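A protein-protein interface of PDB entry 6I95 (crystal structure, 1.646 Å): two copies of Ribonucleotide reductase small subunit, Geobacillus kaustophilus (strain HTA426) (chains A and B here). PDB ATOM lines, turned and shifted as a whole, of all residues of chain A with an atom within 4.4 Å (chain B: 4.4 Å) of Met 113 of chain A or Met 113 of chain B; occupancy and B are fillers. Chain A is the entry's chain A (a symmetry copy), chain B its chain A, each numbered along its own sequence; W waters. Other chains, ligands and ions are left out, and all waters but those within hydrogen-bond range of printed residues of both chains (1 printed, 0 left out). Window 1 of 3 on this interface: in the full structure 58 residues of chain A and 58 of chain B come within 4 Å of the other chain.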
ATOM      1  N   ILE A  90      -4.051  32.348   8.538  1.00  0.00           N
ATOM      2  CA  ILE A  90      -3.685  31.160   9.283  1.00  0.00           C
ATOM      3  C   ILE A  90      -3.370  29.987   8.354  1.00  0.00           C
ATOM      4  O   ILE A  90      -2.730  29.029   8.771  1.00  0.00           O
ATOM      5  CB  ILE A  90      -4.815  30.836  10.285  1.00  0.00           C
ATOM      6  CG1 ILE A  90      -4.383  29.775  11.281  1.00  0.00           C
ATOM      7  CG2 ILE A  90      -6.040  30.437   9.560  1.00  0.00           C
ATOM      8  CD1 ILE A  90      -3.238  30.250  12.193  1.00  0.00           C
ATOM      9  N   LEU A  91      -3.751  30.062   7.079  1.00  0.00           N
ATOM     10  CA  LEU A  91      -3.600  28.891   6.220  1.00  0.00           C
ATOM     11  C   LEU A  91      -2.141  28.465   6.078  1.00  0.00           C
ATOM     12  O   LEU A  91      -1.887  27.259   6.038  1.00  0.00           O
ATOM     13  CB  LEU A  91      -4.235  29.167   4.843  1.00  0.00           C
ATOM     14  CG  LEU A  91      -5.775  29.246   4.825  1.00  0.00           C
ATOM     15  CD1 LEU A  91      -6.296  29.858   3.507  1.00  0.00           C
ATOM     16  CD2 LEU A  91      -6.306  27.843   4.976  1.00  0.00           C
ATOM     17  N   LEU A 109      -6.339  23.460  14.413  1.00  0.00           N
ATOM     18  CA  LEU A 109      -6.376  24.641  13.565  1.00  0.00           C
ATOM     19  C   LEU A 109      -7.617  24.661  12.667  1.00  0.00           C
ATOM     20  O   LEU A 109      -8.014  25.753  12.250  1.00  0.00           O
ATOM     21  CB  LEU A 109      -5.102  24.762  12.721  1.00  0.00           C
ATOM     22  CG  LEU A 109      -3.881  25.255  13.549  1.00  0.00           C
ATOM     23  CD1 LEU A 109      -2.632  25.275  12.667  1.00  0.00           C
ATOM     24  CD2 LEU A 109      -4.112  26.649  14.155  1.00  0.00           C
ATOM     25  N   THR A 110      -8.235  23.515  12.353  1.00  0.00           N
ATOM     26  CA  THR A 110      -9.522  23.608  11.622  1.00  0.00           C
ATOM     27  C   THR A 110     -10.576  24.357  12.454  1.00  0.00           C
ATOM     28  O   THR A 110     -11.390  25.113  11.897  1.00  0.00           O
ATOM     29  CB  THR A 110     -10.077  22.232  11.216  1.00  0.00           C
ATOM     30  OG1 THR A 110     -10.562  21.511  12.368  1.00  0.00           O
ATOM     31  CG2 THR A 110      -9.090  21.427  10.432  1.00  0.00           C
ATOM     32  N   THR A 111     -10.551  24.217  13.787  1.00  0.00           N
ATOM     33  CA  THR A 111     -11.504  24.961  14.605  1.00  0.00           C
ATOM     34  C   THR A 111     -11.103  26.422  14.700  1.00  0.00           C
ATOM     35  O   THR A 111     -11.973  27.297  14.770  1.00  0.00           O
ATOM     36  CB  THR A 111     -11.662  24.362  16.031  1.00  0.00           C
ATOM     37  OG1 THR A 111     -10.503  24.633  16.852  1.00  0.00           O
ATOM     38  CG2 THR A 111     -11.876  22.891  15.959  1.00  0.00           C
ATOM     39  N   PHE A 112      -9.792  26.699  14.712  1.00  0.00           N
ATOM     40  CA  PHE A 112      -9.276  28.061  14.750  1.00  0.00           C
ATOM     41  C   PHE A 112      -9.738  28.836  13.523  1.00  0.00           C
ATOM     42  O   PHE A 112     -10.276  29.951  13.630  1.00  0.00           O
ATOM     43  CB  PHE A 112      -7.741  27.945  14.846  1.00  0.00           C
ATOM     44  CG  PHE A 112      -6.964  29.212  15.163  1.00  0.00           C
ATOM     45  CD1 PHE A 112      -6.006  29.165  16.162  1.00  0.00           C
ATOM     46  CD2 PHE A 112      -7.081  30.374  14.444  1.00  0.00           C
ATOM     47  CE1 PHE A 112      -5.254  30.262  16.470  1.00  0.00           C
ATOM     48  CE2 PHE A 112      -6.300  31.495  14.747  1.00  0.00           C
ATOM     49  CZ  PHE A 112      -5.382  31.426  15.759  1.00  0.00           C
ATOM     50  N   MET A 113      -9.565  28.230  12.356  1.00  0.00           N
ATOM     51  CA  MET A 113      -9.950  28.869  11.098  1.00  0.00           C
ATOM     52  C   MET A 113     -11.447  29.080  11.015  1.00  0.00           C
ATOM     53  O   MET A 113     -11.910  30.135  10.540  1.00  0.00           O
ATOM     54  CB  MET A 113      -9.484  27.989   9.925  1.00  0.00           C
ATOM     55  CG  MET A 113      -7.996  27.886   9.873  1.00  0.00           C
ATOM     56  SD  MET A 113      -7.193  27.096   8.482  1.00  0.00           S
ATOM     57  CE  MET A 113      -7.822  25.497   8.761  1.00  0.00           C
ATOM     58  N   HIS A 114     -12.224  28.064  11.411  1.00  0.00           N
ATOM     59  CA  HIS A 114     -13.674  28.241  11.351  1.00  0.00           C
ATOM     60  C   HIS A 114     -14.160  29.290  12.340  1.00  0.00           C
ATOM     61  O   HIS A 114     -15.105  30.041  12.039  1.00  0.00           O
ATOM     62  CB  HIS A 114     -14.382  26.928  11.588  1.00  0.00           C
ATOM     63  CG  HIS A 114     -15.859  27.093  11.543  1.00  0.00           C
ATOM     64  ND1 HIS A 114     -16.495  27.610  10.433  1.00  0.00           N
ATOM     65  CD2 HIS A 114     -16.810  26.913  12.488  1.00  0.00           C
ATOM     66  CE1 HIS A 114     -17.797  27.692  10.683  1.00  0.00           C
ATOM     67  NE2 HIS A 114     -18.015  27.269  11.923  1.00  0.00           N
ATOM     68  N   ASP A 115     -13.538  29.371  13.524  1.00  0.00           N
ATOM     69  CA  ASP A 115     -13.839  30.462  14.439  1.00  0.00           C
ATOM     70  C   ASP A 115     -13.634  31.807  13.750  1.00  0.00           C
ATOM     71  O   ASP A 115     -14.487  32.698  13.833  1.00  0.00           O
ATOM     72  CB  ASP A 115     -12.958  30.419  15.702  1.00  0.00           C
ATOM     73  CG  ASP A 115     -13.250  29.276  16.619  1.00  0.00           C
ATOM     74  OD1 ASP A 115     -14.273  28.596  16.506  1.00  0.00           O
ATOM     75  OD2 ASP A 115     -12.394  29.042  17.507  1.00  0.00           O
ATOM     76  N   GLU A 116     -12.472  32.000  13.101  1.00  0.00           N
ATOM     77  CA  GLU A 116     -12.207  33.295  12.469  1.00  0.00           C
ATOM     78  C   GLU A 116     -13.234  33.605  11.389  1.00  0.00           C
ATOM     79  O   GLU A 116     -13.638  34.754  11.260  1.00  0.00           O
ATOM     80  CB  GLU A 116     -10.819  33.377  11.839  1.00  0.00           C
ATOM     81  CG  GLU A 116      -9.679  33.108  12.815  1.00  0.00           C
ATOM     82  CD  GLU A 116      -9.600  34.036  13.994  1.00  0.00           C
ATOM     83  OE1 GLU A 116     -10.442  34.957  14.200  1.00  0.00           O
ATOM     84  OE2 GLU A 116      -8.625  33.849  14.721  1.00  0.00           O
ATOM     85  N   ALA A 117     -13.674  32.600  10.630  1.00  0.00           N
ATOM     86  CA  ALA A 117     -14.735  32.802   9.638  1.00  0.00           C
ATOM     87  C   ALA A 117     -15.998  33.360  10.295  1.00  0.00           C
ATOM     88  O   ALA A 117     -16.638  34.290   9.775  1.00  0.00           O
ATOM     89  CB  ALA A 117     -15.054  31.480   8.949  1.00  0.00           C
ATOM     90  N   ILE B  90      -6.840  19.636   1.517  1.00  0.00           N
ATOM     91  CA  ILE B  90      -7.687  20.740   1.116  1.00  0.00           C
ATOM     92  C   ILE B  90      -6.997  22.087   1.329  1.00  0.00           C
ATOM     93  O   ILE B  90      -7.407  23.086   0.748  1.00  0.00           O
ATOM     94  CB  ILE B  90      -9.029  20.634   1.873  1.00  0.00           C
ATOM     95  CG1 ILE B  90     -10.061  21.591   1.304  1.00  0.00           C
ATOM     96  CG2 ILE B  90      -8.818  20.857   3.319  1.00  0.00           C
ATOM     97  CD1 ILE B  90     -10.454  21.247  -0.145  1.00  0.00           C
ATOM     98  N   LEU B  91      -5.914  22.134   2.105  1.00  0.00           N
ATOM     99  CA  LEU B  91      -5.338  23.431   2.446  1.00  0.00           C
ATOM    100  C   LEU B  91      -4.862  24.194   1.211  1.00  0.00           C
ATOM    101  O   LEU B  91      -5.021  25.416   1.184  1.00  0.00           O
ATOM    102  CB  LEU B  91      -4.192  23.244   3.459  1.00  0.00           C
ATOM    103  CG  LEU B  91      -4.622  22.823   4.879  1.00  0.00           C
ATOM    104  CD1 LEU B  91      -3.419  22.329   5.713  1.00  0.00           C
ATOM    105  CD2 LEU B  91      -5.239  24.027   5.545  1.00  0.00           C
ATOM    106  N   LEU B 109     -14.981  26.712   3.063  1.00  0.00           N
ATOM    107  CA  LEU B 109     -13.939  25.706   3.196  1.00  0.00           C
ATOM    108  C   LEU B 109     -13.477  25.550   4.649  1.00  0.00           C
ATOM    109  O   LEU B 109     -12.964  24.479   4.983  1.00  0.00           O
ATOM    110  CB  LEU B 109     -12.746  26.014   2.285  1.00  0.00           C
ATOM    111  CG  LEU B 109     -13.032  25.683   0.792  1.00  0.00           C
ATOM    112  CD1 LEU B 109     -11.834  26.087  -0.068  1.00  0.00           C
ATOM    113  CD2 LEU B 109     -13.348  24.193   0.576  1.00  0.00           C
ATOM    114  N   THR B 110     -13.632  26.562   5.512  1.00  0.00           N
ATOM    115  CA  THR B 110     -13.322  26.299   6.939  1.00  0.00           C
ATOM    116  C   THR B 110     -14.241  25.208   7.510  1.00  0.00           C
ATOM    117  O   THR B 110     -13.800  24.388   8.333  1.00  0.00           O
ATOM    118  CB  THR B 110     -13.424  27.562   7.813  1.00  0.00           C
ATOM    119  OG1 THR B 110     -14.800  27.960   7.985  1.00  0.00           O
ATOM    120  CG2 THR B 110     -12.582  28.684   7.295  1.00  0.00           C
ATOM    121  N   THR B 111     -15.499  25.133   7.056  1.00  0.00           N
ATOM    122  CA  THR B 111     -16.377  24.072   7.539  1.00  0.00           C
ATOM    123  C   THR B 111     -16.014  22.744   6.902  1.00  0.00           C
ATOM    124  O   THR B 111     -16.143  21.696   7.542  1.00  0.00           O
ATOM    125  CB  THR B 111     -17.881  24.383   7.296  1.00  0.00           C
ATOM    126  OG1 THR B 111     -18.231  24.252   5.900  1.00  0.00           O
ATOM    127  CG2 THR B 111     -18.211  25.758   7.756  1.00  0.00           C
ATOM    128  N   PHE B 112     -15.567  22.772   5.638  1.00  0.00           N
ATOM    129  CA  PHE B 112     -15.139  21.574   4.928  1.00  0.00           C
ATOM    130  C   PHE B 112     -13.967  20.923   5.650  1.00  0.00           C
ATOM    131  O   PHE B 112     -13.975  19.712   5.933  1.00  0.00           O
ATOM    132  CB  PHE B 112     -14.791  22.017   3.492  1.00  0.00           C
ATOM    133  CG  PHE B 112     -14.563  20.924   2.461  1.00  0.00           C
ATOM    134  CD1 PHE B 112     -15.211  21.026   1.241  1.00  0.00           C
ATOM    135  CD2 PHE B 112     -13.670  19.897   2.628  1.00  0.00           C
ATOM    136  CE1 PHE B 112     -15.021  20.092   0.263  1.00  0.00           C
ATOM    137  CE2 PHE B 112     -13.462  18.948   1.620  1.00  0.00           C
ATOM    138  CZ  PHE B 112     -14.138  19.059   0.436  1.00  0.00           C
ATOM    139  N   MET B 113     -12.970  21.732   5.986  1.00  0.00           N
ATOM    140  CA  MET B 113     -11.776  21.233   6.668  1.00  0.00           C
ATOM    141  C   MET B 113     -12.103  20.705   8.048  1.00  0.00           C
ATOM    142  O   MET B 113     -11.564  19.664   8.470  1.00  0.00           O
ATOM    143  CB  MET B 113     -10.748  22.372   6.778  1.00  0.00           C
ATOM    144  CG  MET B 113     -10.274  22.815   5.434  1.00  0.00           C
ATOM    145  SD  MET B 113      -8.923  23.980   5.292  1.00  0.00           S
ATOM    146  CE  MET B 113      -9.732  25.329   6.036  1.00  0.00           C
ATOM    147  N   HIS B 114     -12.935  21.442   8.797  1.00  0.00           N
ATOM    148  CA  HIS B 114     -13.276  20.953  10.132  1.00  0.00           C
ATOM    149  C   HIS B 114     -14.101  19.678  10.076  1.00  0.00           C
ATOM    150  O   HIS B 114     -13.939  18.790  10.933  1.00  0.00           O
ATOM    151  CB  HIS B 114     -14.007  22.017  10.918  1.00  0.00           C
ATOM    152  CG  HIS B 114     -14.372  21.532  12.275  1.00  0.00           C
ATOM    153  ND1 HIS B 114     -13.419  21.070  13.159  1.00  0.00           N
ATOM    154  CD2 HIS B 114     -15.575  21.338  12.863  1.00  0.00           C
ATOM    155  CE1 HIS B 114     -14.025  20.657  14.267  1.00  0.00           C
ATOM    156  NE2 HIS B 114     -15.335  20.815  14.114  1.00  0.00           N
ATOM    157  N   ASP B 115     -14.992  19.550   9.084  1.00  0.00           N
ATOM    158  CA  ASP B 115     -15.684  18.286   8.875  1.00  0.00           C
ATOM    159  C   ASP B 115     -14.680  17.150   8.703  1.00  0.00           C
ATOM    160  O   ASP B 115     -14.813  16.089   9.322  1.00  0.00           O
ATOM    161  CB  ASP B 115     -16.598  18.324   7.635  1.00  0.00           C
ATOM    162  CG  ASP B 115     -17.793  19.208   7.776  1.00  0.00           C
ATOM    163  OD1 ASP B 115     -18.151  19.649   8.872  1.00  0.00           O
ATOM    164  OD2 ASP B 115     -18.411  19.484   6.719  1.00  0.00           O
ATOM    165  N   GLU B 116     -13.685  17.332   7.818  1.00  0.00           N
ATOM    166  CA  GLU B 116     -12.727  16.250   7.579  1.00  0.00           C
ATOM    167  C   GLU B 116     -11.966  15.894   8.849  1.00  0.00           C
ATOM    168  O   GLU B 116     -11.709  14.719   9.082  1.00  0.00           O
ATOM    169  CB  GLU B 116     -11.706  16.586   6.496  1.00  0.00           C
ATOM    170  CG  GLU B 116     -12.327  16.945   5.150  1.00  0.00           C
ATOM    171  CD  GLU B 116     -13.185  15.882   4.525  1.00  0.00           C
ATOM    172  OE1 GLU B 116     -13.422  14.773   5.087  1.00  0.00           O
ATOM    173  OE2 GLU B 116     -13.607  16.165   3.404  1.00  0.00           O
ATOM    174  N   ALA B 117     -11.623  16.882   9.677  1.00  0.00           N
ATOM    175  CA  ALA B 117     -10.979  16.608  10.965  1.00  0.00           C
ATOM    176  C   ALA B 117     -11.842  15.680  11.821  1.00  0.00           C
ATOM    177  O   ALA B 117     -11.344  14.725  12.442  1.00  0.00           O
ATOM    178  CB  ALA B 117     -10.736  17.916  11.708  1.00  0.00           C
HETATM  179  O   HOH W   1      -2.312  26.536   2.798  1.00  0.00           O
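Thr 110 of chain A touches Met 113 of chain B, and with the chains exchanged Met 113 of chain A touches Thr 110 of chain B. Thr 110 of chain A touches Ala 117 of chain B, and with the chains exchanged Ala 117 of chain A touches Thr 110 of chain B. Thr 111 of chain A touches His 114 of chain B, and with the chains exchanged His 114 of chain A touches Thr 111 of chain B. Met 113 of chain A touches its own counterpart, Met 113 of chain B. Of the 9 pairs that touch across the chains among the printed residues, 9 have their exchanged pair printed and touching as well.
Printed residues of chain B that touch a printed residue of chain A: Thr 110, Thr 111, Met 113, His 114 and Ala 117. Of the 11 printed residues of chain A, 5 touch a printed residue of chain B. Hydrophobic or aromatic side chains of chain A that line the printed part of chain B: Met 113, His 114 and Ala 117.
Of the printed residues of chain B, Met 113 of chain A touches Thr 110 and Met 113. Printed residues of chain A within 4 Å of Met 113 of chain B: Thr 110 and Met 113. Printed residues of chain B within 4 Å of Ala 117 of chain A: Thr 110. Of the printed residues of chain A, Thr 110 of chain B touches Met 113 (3.6 Å), His 114 (3.0 Å) and Ala 117 (3.7 Å). Printed residues of chain A within 4 Å of Ala 117 of chain B: Thr 110. Of the printed residues of chain B, Thr 110 of chain A touches Met 113 (3.6 Å), His 114 (3.0 Å) and Ala 117 (3.7 Å). Of the printed residues of chain B, Thr 111 of chain A touches His 114 (3.5 Å). Ile 90 of chain A touches none of the printed residues of chain B. Glu 116 of chain B touches none of the printed residues of chain A. The nearest printed residue of chain B that does not touch Thr 110 of chain A is Thr 110 of chain B (4.4 Å).
The side-chain hydroxyl (OG1) of Thr 110 of chain A lies within hydrogen-bond range of a ring nitrogen (ND1) of His 114 of chain B. ND1 of His 114 of chain A lies within hydrogen-bond range of OG1 of Thr 110 of chain B, 3.0 Å away.
Water W1 bridges the backbone carbonyl oxygen (O) of Leu 91 of chain B (3.3 Å) and the backbone carbonyl oxygen (O) of Leu 91 of chain A (3.3 Å).
Among the printed residues, merely in contact across the chains: Thr 110 of chain A with Met 113 of chain B (3.6 Å), Thr 110 of chain A with Ala 117 of chain B (3.7 Å), Thr 111 of chain A with His 114 of chain B (3.5 Å), Met 113 of chain A with Thr 110 of chain B (3.6 Å), Met 113 of chain A with Met 113 of chain B (3.3 Å), His 114 of chain A with Thr 111 of chain B (3.5 Å) and Ala 117 of chain A with Thr 110 of chain B (3.7 Å).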
